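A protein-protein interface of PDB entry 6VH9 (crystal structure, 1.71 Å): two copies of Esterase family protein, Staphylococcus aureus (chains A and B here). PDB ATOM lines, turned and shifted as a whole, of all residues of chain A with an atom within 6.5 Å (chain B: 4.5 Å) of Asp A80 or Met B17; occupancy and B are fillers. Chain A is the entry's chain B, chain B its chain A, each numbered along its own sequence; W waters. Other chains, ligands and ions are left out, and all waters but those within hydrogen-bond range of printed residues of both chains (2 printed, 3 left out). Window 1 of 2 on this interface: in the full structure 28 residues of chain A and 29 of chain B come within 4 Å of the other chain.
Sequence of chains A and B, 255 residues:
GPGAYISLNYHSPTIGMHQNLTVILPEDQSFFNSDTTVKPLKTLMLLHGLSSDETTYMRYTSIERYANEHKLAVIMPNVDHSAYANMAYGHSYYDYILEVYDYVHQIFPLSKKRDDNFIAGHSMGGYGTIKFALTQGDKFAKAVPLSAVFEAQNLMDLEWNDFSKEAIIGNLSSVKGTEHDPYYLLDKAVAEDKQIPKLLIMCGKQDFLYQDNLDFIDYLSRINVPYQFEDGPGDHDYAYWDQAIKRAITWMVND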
ATOM      1  N   GLN A  19      -6.971   8.049  20.028  1.00  0.00           N
ATOM      2  CA  GLN A  19      -6.554   8.767  18.810  1.00  0.00           C
ATOM      3  C   GLN A  19      -7.176   8.041  17.620  1.00  0.00           C
ATOM      4  O   GLN A  19      -7.279   6.853  17.675  1.00  0.00           O
ATOM      5  CB  GLN A  19      -5.034   8.746  18.722  1.00  0.00           C
ATOM      6  CG  GLN A  19      -4.452   9.695  17.693  1.00  0.00           C
ATOM      7  CD  GLN A  19      -4.344  11.113  18.189  1.00  0.00           C
ATOM      8  OE1 GLN A  19      -5.057  11.539  19.068  1.00  0.00           O
ATOM      9  NE2 GLN A  19      -3.440  11.859  17.601  1.00  0.00           N
ATOM     10  N   HIS A  48       0.283  13.243   7.031  1.00  0.00           N
ATOM     11  CA  HIS A  48      -0.369  14.487   6.652  1.00  0.00           C
ATOM     12  C   HIS A  48       0.516  15.698   6.980  1.00  0.00           C
ATOM     13  O   HIS A  48       1.462  15.618   7.769  1.00  0.00           O
ATOM     14  CB  HIS A  48      -1.717  14.618   7.377  1.00  0.00           C
ATOM     15  CG  HIS A  48      -1.585  14.733   8.870  1.00  0.00           C
ATOM     16  ND1 HIS A  48      -1.153  15.887   9.494  1.00  0.00           N
ATOM     17  CD2 HIS A  48      -1.838  13.841   9.861  1.00  0.00           C
ATOM     18  CE1 HIS A  48      -1.144  15.701  10.803  1.00  0.00           C
ATOM     19  NE2 HIS A  48      -1.543  14.466  11.052  1.00  0.00           N
ATOM     20  N   GLY A  49       0.166  16.840   6.382  1.00  0.00           N
ATOM     21  CA  GLY A  49       0.860  18.089   6.622  1.00  0.00           C
ATOM     22  C   GLY A  49       0.216  18.885   7.744  1.00  0.00           C
ATOM     23  O   GLY A  49      -0.722  18.444   8.408  1.00  0.00           O
ATOM     24  N   LEU A  50       0.733  20.086   7.953  1.00  0.00           N
ATOM     25  CA  LEU A  50       0.255  20.909   9.050  1.00  0.00           C
ATOM     26  C   LEU A  50      -1.156  21.390   8.747  1.00  0.00           C
ATOM     27  O   LEU A  50      -1.419  21.893   7.651  1.00  0.00           O
ATOM     28  CB  LEU A  50       1.206  22.096   9.255  1.00  0.00           C
ATOM     29  CG  LEU A  50       0.911  23.086  10.378  1.00  0.00           C
ATOM     30  CD1 LEU A  50       0.875  22.358  11.699  1.00  0.00           C
ATOM     31  CD2 LEU A  50       1.995  24.203  10.402  1.00  0.00           C
ATOM     32  N   SER A  51      -2.061  21.224   9.717  1.00  0.00           N
ATOM     33  CA  SER A  51      -3.482  21.567   9.692  1.00  0.00           C
ATOM     34  C   SER A  51      -4.349  20.410   9.196  1.00  0.00           C
ATOM     35  O   SER A  51      -5.564  20.466   9.361  1.00  0.00           O
ATOM     36  CB  SER A  51      -3.800  22.840   8.881  1.00  0.00           C
ATOM     37  OG  SER A  51      -4.068  22.554   7.517  1.00  0.00           O
ATOM     38  N   SER A  52      -3.765  19.367   8.602  1.00  0.00           N
ATOM     39  CA  SER A  52      -4.522  18.190   8.189  1.00  0.00           C
ATOM     40  C   SER A  52      -4.600  17.171   9.332  1.00  0.00           C
ATOM     41  O   SER A  52      -4.070  17.383  10.427  1.00  0.00           O
ATOM     42  CB  SER A  52      -3.909  17.574   6.933  1.00  0.00           C
ATOM     43  OG  SER A  52      -3.950  18.480   5.847  1.00  0.00           O
ATOM     44  N   ASP A  53      -5.293  16.061   9.092  1.00  0.00           N
ATOM     45  CA  ASP A  53      -5.336  14.983  10.077  1.00  0.00           C
ATOM     46  C   ASP A  53      -5.536  13.661   9.334  1.00  0.00           C
ATOM     47  O   ASP A  53      -5.281  13.573   8.129  1.00  0.00           O
ATOM     48  CB  ASP A  53      -6.406  15.267  11.151  1.00  0.00           C
ATOM     49  CG  ASP A  53      -7.842  15.185  10.631  1.00  0.00           C
ATOM     50  OD1 ASP A  53      -8.075  14.832   9.447  1.00  0.00           O
ATOM     51  OD2 ASP A  53      -8.748  15.478  11.448  1.00  0.00           O
ATOM     52  N   ASN A  78      -2.794  10.406  12.739  1.00  0.00           N
ATOM     53  CA  ASN A  78      -2.961  11.807  13.107  1.00  0.00           C
ATOM     54  C   ASN A  78      -1.883  12.200  14.107  1.00  0.00           C
ATOM     55  O   ASN A  78      -1.746  11.546  15.145  1.00  0.00           O
ATOM     56  CB  ASN A  78      -4.353  12.016  13.723  1.00  0.00           C
ATOM     57  CG  ASN A  78      -4.573  13.430  14.238  1.00  0.00           C
ATOM     58  OD1 ASN A  78      -4.087  14.393  13.647  1.00  0.00           O
ATOM     59  ND2 ASN A  78      -5.270  13.558  15.356  1.00  0.00           N
ATOM     60  N   VAL A  79      -1.135  13.282  13.820  1.00  0.00           N
ATOM     61  CA  VAL A  79      -0.105  13.755  14.755  1.00  0.00           C
ATOM     62  C   VAL A  79      -0.250  15.250  15.037  1.00  0.00           C
ATOM     63  O   VAL A  79       0.670  15.880  15.576  1.00  0.00           O
ATOM     64  CB  VAL A  79       1.328  13.453  14.263  1.00  0.00           C
ATOM     65  CG1 VAL A  79       1.529  11.964  13.983  1.00  0.00           C
ATOM     66  CG2 VAL A  79       1.670  14.309  13.053  1.00  0.00           C
ATOM     67  N   ASP A  80      -1.386  15.843  14.674  1.00  0.00           N
ATOM     68  CA  ASP A  80      -1.705  17.182  15.168  1.00  0.00           C
ATOM     69  C   ASP A  80      -0.672  18.177  14.628  1.00  0.00           C
ATOM     70  O   ASP A  80      -0.297  18.097  13.453  1.00  0.00           O
ATOM     71  CB  ASP A  80      -1.740  17.137  16.708  1.00  0.00           C
ATOM     72  CG  ASP A  80      -2.470  18.306  17.338  1.00  0.00           C
ATOM     73  OD1 ASP A  80      -3.640  18.118  17.759  1.00  0.00           O
ATOM     74  OD2 ASP A  80      -1.852  19.390  17.475  1.00  0.00           O
ATOM     75  N   HIS A  81      -0.189  19.094  15.477  1.00  0.00           N
ATOM     76  CA  HIS A  81       0.804  20.102  15.111  1.00  0.00           C
ATOM     77  C   HIS A  81       2.217  19.731  15.550  1.00  0.00           C
ATOM     78  O   HIS A  81       3.041  20.619  15.767  1.00  0.00           O
ATOM     79  CB  HIS A  81       0.457  21.439  15.749  1.00  0.00           C
ATOM     80  CG  HIS A  81      -0.594  22.214  15.024  1.00  0.00           C
ATOM     81  ND1 HIS A  81      -0.772  23.567  15.214  1.00  0.00           N
ATOM     82  CD2 HIS A  81      -1.529  21.831  14.120  1.00  0.00           C
ATOM     83  CE1 HIS A  81      -1.769  23.990  14.455  1.00  0.00           C
ATOM     84  NE2 HIS A  81      -2.247  22.955  13.785  1.00  0.00           N
ATOM     85  N   SER A  82       2.501  18.445  15.712  1.00  0.00           N
ATOM     86  CA  SER A  82       3.723  17.969  16.363  1.00  0.00           C
ATOM     87  C   SER A  82       4.980  17.979  15.497  1.00  0.00           C
ATOM     88  O   SER A  82       6.077  17.791  16.049  1.00  0.00           O
ATOM     89  CB  SER A  82       3.461  16.565  16.878  1.00  0.00           C
ATOM     90  OG  SER A  82       3.446  15.705  15.759  1.00  0.00           O
ATOM     91  N   ALA A  83       4.843  18.083  14.177  1.00  0.00           N
ATOM     92  CA  ALA A  83       5.954  17.884  13.242  1.00  0.00           C
ATOM     93  C   ALA A  83       6.623  16.519  13.413  1.00  0.00           C
ATOM     94  O   ALA A  83       7.822  16.365  13.153  1.00  0.00           O
ATOM     95  CB  ALA A  83       6.993  19.006  13.346  1.00  0.00           C
ATOM     96  N   TYR A  84       5.859  15.515  13.856  1.00  0.00           N
ATOM     97  CA  TYR A  84       6.328  14.130  13.989  1.00  0.00           C
ATOM     98  C   TYR A  84       7.473  14.015  14.985  1.00  0.00           C
ATOM     99  O   TYR A  84       8.327  13.138  14.867  1.00  0.00           O
ATOM    100  CB  TYR A  84       6.706  13.544  12.619  1.00  0.00           C
ATOM    101  CG  TYR A  84       5.491  13.525  11.737  1.00  0.00           C
ATOM    102  CD1 TYR A  84       4.611  12.441  11.747  1.00  0.00           C
ATOM    103  CD2 TYR A  84       5.161  14.636  10.966  1.00  0.00           C
ATOM    104  CE1 TYR A  84       3.467  12.441  10.967  1.00  0.00           C
ATOM    105  CE2 TYR A  84       4.012  14.656  10.194  1.00  0.00           C
ATOM    106  CZ  TYR A  84       3.169  13.552  10.196  1.00  0.00           C
ATOM    107  OH  TYR A  84       2.020  13.583   9.442  1.00  0.00           O
ATOM    108  N   MET A  87       7.620  15.685  21.435  1.00  0.00           N
ATOM    109  CA  MET A  87       7.550  17.116  21.695  1.00  0.00           C
ATOM    110  C   MET A  87       8.138  17.479  23.055  1.00  0.00           C
ATOM    111  O   MET A  87       7.951  16.764  24.043  1.00  0.00           O
ATOM    112  CB  MET A  87       6.100  17.598  21.620  1.00  0.00           C
ATOM    113  CG  MET A  87       5.455  17.404  20.254  1.00  0.00           C
ATOM    114  SD  MET A  87       3.665  17.655  20.290  1.00  0.00           S
ATOM    115  CE  MET A  87       3.540  19.432  20.380  1.00  0.00           C
ATOM    116  N   TYR A  93       5.117  12.054  19.728  1.00  0.00           N
ATOM    117  CA  TYR A  93       4.541  11.682  18.433  1.00  0.00           C
ATOM    118  C   TYR A  93       5.538  11.000  17.508  1.00  0.00           C
ATOM    119  O   TYR A  93       5.115  10.289  16.591  1.00  0.00           O
ATOM    120  CB  TYR A  93       3.941  12.901  17.735  1.00  0.00           C
ATOM    121  CG  TYR A  93       2.483  13.157  18.072  1.00  0.00           C
ATOM    122  CD1 TYR A  93       1.502  12.240  17.731  1.00  0.00           C
ATOM    123  CD2 TYR A  93       2.093  14.329  18.735  1.00  0.00           C
ATOM    124  CE1 TYR A  93       0.156  12.491  18.014  1.00  0.00           C
ATOM    125  CE2 TYR A  93       0.766  14.592  19.012  1.00  0.00           C
ATOM    126  CZ  TYR A  93      -0.203  13.659  18.659  1.00  0.00           C
ATOM    127  OH  TYR A  93      -1.528  13.927  18.938  1.00  0.00           O
ATOM    128  N   MET A 124       4.710  19.251   6.180  1.00  0.00           N
ATOM    129  CA  MET A 124       5.113  18.734   7.487  1.00  0.00           C
ATOM    130  C   MET A 124       5.239  17.214   7.479  1.00  0.00           C
ATOM    131  O   MET A 124       6.093  16.652   8.180  1.00  0.00           O
ATOM    132  CB  MET A 124       4.116  19.183   8.564  1.00  0.00           C
ATOM    133  CG  MET A 124       4.518  18.759   9.986  1.00  0.00           C
ATOM    134  SD  MET A 124       3.273  19.154  11.223  1.00  0.00           S
ATOM    135  CE  MET A 124       2.129  17.768  11.053  1.00  0.00           C
ATOM    136  N   TRP A 160       1.972  29.929  11.235  1.00  0.00           N
ATOM    137  CA  TRP A 160       0.682  29.221  10.998  1.00  0.00           C
ATOM    138  C   TRP A 160      -0.264  29.390  12.189  1.00  0.00           C
ATOM    139  O   TRP A 160       0.175  29.468  13.293  1.00  0.00           O
ATOM    140  CB  TRP A 160       0.822  27.747  10.529  1.00  0.00           C
ATOM    141  CG  TRP A 160      -0.480  26.999  10.369  1.00  0.00           C
ATOM    142  CD1 TRP A 160      -1.004  26.051  11.205  1.00  0.00           C
ATOM    143  CD2 TRP A 160      -1.558  27.336   9.475  1.00  0.00           C
ATOM    144  NE1 TRP A 160      -2.275  25.709  10.841  1.00  0.00           N
ATOM    145  CE2 TRP A 160      -2.632  26.464   9.759  1.00  0.00           C
ATOM    146  CE3 TRP A 160      -1.712  28.262   8.439  1.00  0.00           C
ATOM    147  CZ2 TRP A 160      -3.828  26.499   9.045  1.00  0.00           C
ATOM    148  CZ3 TRP A 160      -2.885  28.279   7.718  1.00  0.00           C
ATOM    149  CH2 TRP A 160      -3.931  27.408   8.020  1.00  0.00           C
ATOM    150  N   ASN A 161      -1.532  29.572  11.882  1.00  0.00           N
ATOM    151  CA  ASN A 161      -2.663  29.631  12.818  1.00  0.00           C
ATOM    152  C   ASN A 161      -2.521  28.620  13.961  1.00  0.00           C
ATOM    153  O   ASN A 161      -2.508  27.439  13.688  1.00  0.00           O
ATOM    154  CB  ASN A 161      -3.904  29.294  12.007  1.00  0.00           C
ATOM    155  CG  ASN A 161      -5.164  29.451  12.804  1.00  0.00           C
ATOM    156  OD1 ASN A 161      -5.095  29.750  13.978  1.00  0.00           O
ATOM    157  ND2 ASN A 161      -6.295  29.249  12.161  1.00  0.00           N
ATOM    158  N   ASP A 162      -2.404  29.130  15.179  1.00  0.00           N
ATOM    159  CA  ASP A 162      -2.398  28.388  16.443  1.00  0.00           C
ATOM    160  C   ASP A 162      -1.213  27.433  16.587  1.00  0.00           C
ATOM    161  O   ASP A 162      -1.217  26.577  17.480  1.00  0.00           O
ATOM    162  CB  ASP A 162      -3.707  27.601  16.649  1.00  0.00           C
ATOM    163  CG  ASP A 162      -4.143  27.561  18.110  1.00  0.00           C
ATOM    164  OD1 ASP A 162      -3.961  28.571  18.823  1.00  0.00           O
ATOM    165  OD2 ASP A 162      -4.648  26.511  18.561  1.00  0.00           O
ATOM    166  N   TYR B  10     -14.086  19.126  10.732  1.00  0.00           N
ATOM    167  CA  TYR B  10     -13.976  20.419  10.026  1.00  0.00           C
ATOM    168  C   TYR B  10     -12.684  21.121  10.411  1.00  0.00           C
ATOM    169  O   TYR B  10     -12.161  20.878  11.460  1.00  0.00           O
ATOM    170  CB  TYR B  10     -15.192  21.303  10.277  1.00  0.00           C
ATOM    171  CG  TYR B  10     -15.241  21.990  11.610  1.00  0.00           C
ATOM    172  CD1 TYR B  10     -15.901  21.431  12.677  1.00  0.00           C
ATOM    173  CD2 TYR B  10     -14.650  23.214  11.801  1.00  0.00           C
ATOM    174  CE1 TYR B  10     -15.963  22.072  13.900  1.00  0.00           C
ATOM    175  CE2 TYR B  10     -14.698  23.867  13.015  1.00  0.00           C
ATOM    176  CZ  TYR B  10     -15.365  23.304  14.072  1.00  0.00           C
ATOM    177  OH  TYR B  10     -15.392  23.952  15.266  1.00  0.00           O
ATOM    178  N   HIS B  11     -12.199  21.956   9.510  1.00  0.00           N
ATOM    179  CA  HIS B  11     -10.976  22.709   9.785  1.00  0.00           C
ATOM    180  C   HIS B  11     -11.321  23.886  10.688  1.00  0.00           C
ATOM    181  O   HIS B  11     -12.042  24.804  10.279  1.00  0.00           O
ATOM    182  CB  HIS B  11     -10.323  23.193   8.491  1.00  0.00           C
ATOM    183  CG  HIS B  11      -8.992  23.845   8.711  1.00  0.00           C
ATOM    184  ND1 HIS B  11      -8.842  24.987   9.468  1.00  0.00           N
ATOM    185  CD2 HIS B  11      -7.751  23.509   8.291  1.00  0.00           C
ATOM    186  CE1 HIS B  11      -7.568  25.330   9.498  1.00  0.00           C
ATOM    187  NE2 HIS B  11      -6.883  24.443   8.800  1.00  0.00           N
ATOM    188  N   SER B  12     -10.785  23.882  11.909  1.00  0.00           N
ATOM    189  CA  SER B  12     -11.143  24.893  12.894  1.00  0.00           C
ATOM    190  C   SER B  12     -10.271  26.129  12.723  1.00  0.00           C
ATOM    191  O   SER B  12      -9.040  26.014  12.778  1.00  0.00           O
ATOM    192  CB  SER B  12     -10.962  24.358  14.300  1.00  0.00           C
ATOM    193  OG  SER B  12     -11.021  25.428  15.221  1.00  0.00           O
ATOM    194  N   ILE B  15      -8.160  26.556  16.275  1.00  0.00           N
ATOM    195  CA  ILE B  15      -7.017  25.702  16.606  1.00  0.00           C
ATOM    196  C   ILE B  15      -6.180  25.330  15.381  1.00  0.00           C
ATOM    197  O   ILE B  15      -5.183  24.603  15.513  1.00  0.00           O
ATOM    198  CB  ILE B  15      -7.434  24.443  17.399  1.00  0.00           C
ATOM    199  CG1 ILE B  15      -8.425  23.555  16.642  1.00  0.00           C
ATOM    200  CG2 ILE B  15      -7.999  24.837  18.780  1.00  0.00           C
ATOM    201  CD1 ILE B  15      -8.878  22.325  17.466  1.00  0.00           C
ATOM    202  N   GLY B  16      -6.505  25.864  14.208  1.00  0.00           N
ATOM    203  CA  GLY B  16      -5.621  25.709  13.062  1.00  0.00           C
ATOM    204  C   GLY B  16      -5.465  24.298  12.535  1.00  0.00           C
ATOM    205  O   GLY B  16      -4.386  23.950  12.030  1.00  0.00           O
ATOM    206  N   MET B  17      -6.524  23.486  12.595  1.00  0.00           N
ATOM    207  CA  MET B  17      -6.418  22.113  12.123  1.00  0.00           C
ATOM    208  C   MET B  17      -7.809  21.510  11.985  1.00  0.00           C
ATOM    209  O   MET B  17      -8.777  21.964  12.603  1.00  0.00           O
ATOM    210  CB  MET B  17      -5.547  21.257  13.059  1.00  0.00           C
ATOM    211  CG  MET B  17      -6.104  21.138  14.446  1.00  0.00           C
ATOM    212  SD  MET B  17      -5.065  20.064  15.457  1.00  0.00           S
ATOM    213  CE  MET B  17      -5.781  20.395  17.059  1.00  0.00           C
ATOM    214  N   HIS B  18      -7.885  20.493  11.142  1.00  0.00           N
ATOM    215  CA  HIS B  18      -9.026  19.594  11.159  1.00  0.00           C
ATOM    216  C   HIS B  18      -9.124  18.921  12.521  1.00  0.00           C
ATOM    217  O   HIS B  18      -8.111  18.585  13.147  1.00  0.00           O
ATOM    218  CB  HIS B  18      -8.867  18.551  10.067  1.00  0.00           C
ATOM    219  CG  HIS B  18      -9.145  19.088   8.706  1.00  0.00           C
ATOM    220  ND1 HIS B  18      -8.235  19.861   8.013  1.00  0.00           N
ATOM    221  CD2 HIS B  18     -10.243  18.996   7.921  1.00  0.00           C
ATOM    222  CE1 HIS B  18      -8.754  20.199   6.845  1.00  0.00           C
ATOM    223  NE2 HIS B  18      -9.972  19.691   6.768  1.00  0.00           N
ATOM    224  N   GLN B  19     -10.353  18.772  12.975  1.00  0.00           N
ATOM    225  CA  GLN B  19     -10.632  18.197  14.302  1.00  0.00           C
ATOM    226  C   GLN B  19     -12.009  17.561  14.255  1.00  0.00           C
ATOM    227  O   GLN B  19     -12.860  18.063  13.569  1.00  0.00           O
ATOM    228  CB  GLN B  19     -10.656  19.317  15.335  1.00  0.00           C
ATOM    229  CG  GLN B  19     -10.615  18.841  16.772  1.00  0.00           C
ATOM    230  CD  GLN B  19      -9.224  18.557  17.269  1.00  0.00           C
ATOM    231  OE1 GLN B  19      -8.328  18.325  16.509  1.00  0.00           O
ATOM    232  NE2 GLN B  19      -9.059  18.535  18.569  1.00  0.00           N
ATOM    233  N   HIS B  91      -2.473  24.490  21.770  1.00  0.00           N
ATOM    234  CA  HIS B  91      -3.615  25.046  21.063  1.00  0.00           C
ATOM    235  C   HIS B  91      -4.493  25.880  21.979  1.00  0.00           C
ATOM    236  O   HIS B  91      -4.472  25.745  23.206  1.00  0.00           O
ATOM    237  CB  HIS B  91      -4.480  23.941  20.452  1.00  0.00           C
ATOM    238  CG  HIS B  91      -3.820  23.188  19.342  1.00  0.00           C
ATOM    239  ND1 HIS B  91      -3.774  23.658  18.045  1.00  0.00           N
ATOM    240  CD2 HIS B  91      -3.215  21.975  19.328  1.00  0.00           C
ATOM    241  CE1 HIS B  91      -3.166  22.765  17.279  1.00  0.00           C
ATOM    242  NE2 HIS B  91      -2.821  21.734  18.032  1.00  0.00           N
ATOM    243  N   TYR B  93      -7.472  25.888  23.265  1.00  0.00           N
ATOM    244  CA  TYR B  93      -8.598  24.982  23.442  1.00  0.00           C
ATOM    245  C   TYR B  93      -9.721  25.574  24.290  1.00  0.00           C
ATOM    246  O   TYR B  93     -10.863  25.130  24.156  1.00  0.00           O
ATOM    247  CB  TYR B  93      -8.117  23.660  24.036  1.00  0.00           C
ATOM    248  CG  TYR B  93      -7.695  22.630  23.005  1.00  0.00           C
ATOM    249  CD1 TYR B  93      -8.628  22.091  22.121  1.00  0.00           C
ATOM    250  CD2 TYR B  93      -6.380  22.172  22.933  1.00  0.00           C
ATOM    251  CE1 TYR B  93      -8.267  21.138  21.186  1.00  0.00           C
ATOM    252  CE2 TYR B  93      -6.006  21.197  22.013  1.00  0.00           C
ATOM    253  CZ  TYR B  93      -6.973  20.679  21.143  1.00  0.00           C
ATOM    254  OH  TYR B  93      -6.637  19.716  20.214  1.00  0.00           O
HETATM  255  O   HOH W   1      -4.223  18.803  20.352  1.00  0.00           O
HETATM  256  O   HOH W   2      -7.994  15.556  14.172  1.00  0.00           O
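A ring nitrogen (NE2) of His A81 sits at hydrogen-bond distance from the backbone carbonyl oxygen (O) of Gly B16 (2.9 Å).
The indole nitrogen (NE1) of Trp A160 is in hydrogen-bond range of the backbone carbonyl oxygen (O) of Gly B16, at 3.0 Å.
The backbone carbonyl oxygen (O) of Ser A51 is in hydrogen-bond range of the backbone NH (N) of His B18, 2.9 Å away.
The side-chain carboxylate (OD2) of Asp A80 sits at hydrogen-bond distance from a ring nitrogen (NE2) of His B91.
ND1 of His B91 sits at hydrogen-bond distance from OD2 of Asp A162, 3.0 Å away.
The side-chain sulfur (SD) of Met B17 sits close to the side-chain carboxylate (OD1) of Asp A80, 3.3 Å away.
The backbone NH of Gln B19 is in hydrogen-bond range of the backbone carbonyl oxygen of Tyr B10.
The side-chain hydroxyl of Ser B12 is in hydrogen-bond range of the backbone NH of Ile B15 (3.3 Å).
O of Met B17 sits at hydrogen-bond distance from N of Ser B12, at 2.9 Å.
ND1 of His B91 sits at hydrogen-bond distance from O of Ile B15, 3.0 Å away.
The side-chain amide nitrogen (NE2) of Gln B19 is in hydrogen-bond range of the side-chain hydroxyl (OH) of Tyr B93 (3.2 Å).
The backbone NH of Asp A80 lies within hydrogen-bond range of the side-chain amide oxygen of Asn A78 (3.2 Å).
Ser A51 touches His B11 (CB to NE2, 3.5 Å).
CB of Ser A51 touches O of Gly B16 (3.4 Å).
Ser A51 touches Met B17 (O to CA, 3.3 Å).
Asp A53 touches His B18.
N of Gln B19 touches OD2 of Asp A53 (3.97 Å).
Ile B15 touches His A81.
CE1 of His B91 touches ND1 of His A81, at 3.3 Å.
CZ2 of Trp A160 touches NE2 of His B11, 3.7 Å away.
Gly B16 touches Asn A161 (CA to O, 3.6 Å).
OD2 of Asp A162 touches CA of Ile B15, at 3.2 Å.
Asp A80 touches just these residues of chain B: Met B17 and His B91.
Printed residues of chain A within 4 Å of Met B17: Ser A51, Asp A80 and His A81.
Of the printed residues of chain B, Asp A162 touches Ile B15 (3.2 Å) and His B91 (3.0 Å).
Of the printed residues of chain A, His B91 touches Asp A80 (2.6 Å), His A81 (3.3 Å) and Asp A162 (3.0 Å).
Printed residues of chain A within 4 Å of His B11: Ser A51 (3.5 Å) and Trp A160 (3.7 Å).
Printed residues of chain A within 4 Å of Ile B15: His A81 (3.6 Å) and Asp A162 (3.2 Å).
Tyr A84 touches none of the printed residues of chain B.
The nearest residue of chain B that does not touch Asp A80 is Tyr B93 (4.2 Å).
The nearest residue of chain A that does not touch Met B17 is Ser A52 (4.9 Å).
Of the 20 printed residues of chain A, 7 touch a printed residue of chain B.
Of the 10 printed residues of chain B, 7 touch a printed residue of chain A.
Printed residues of chain B that touch a printed residue of chain A: His B11, Ile B15, Gly B16, Met B17, His B18, Gln B19 and His B91.
Among the printed residues, no Asp or Glu carboxylate lies within 4 Å of a Lys or Arg side-chain nitrogen of the other chain.
2 positions are printed for both chains.
Of the 17 pairs that touch across the chains among the printed residues, none has its exchanged pair printed and touching as well.
Water W1 bridges OH of Tyr B93 (2.6 Å) and OD1 of Asp A80 (2.7 Å).
Water W2 bridges OD2 of Asp A53 and O of His B18.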
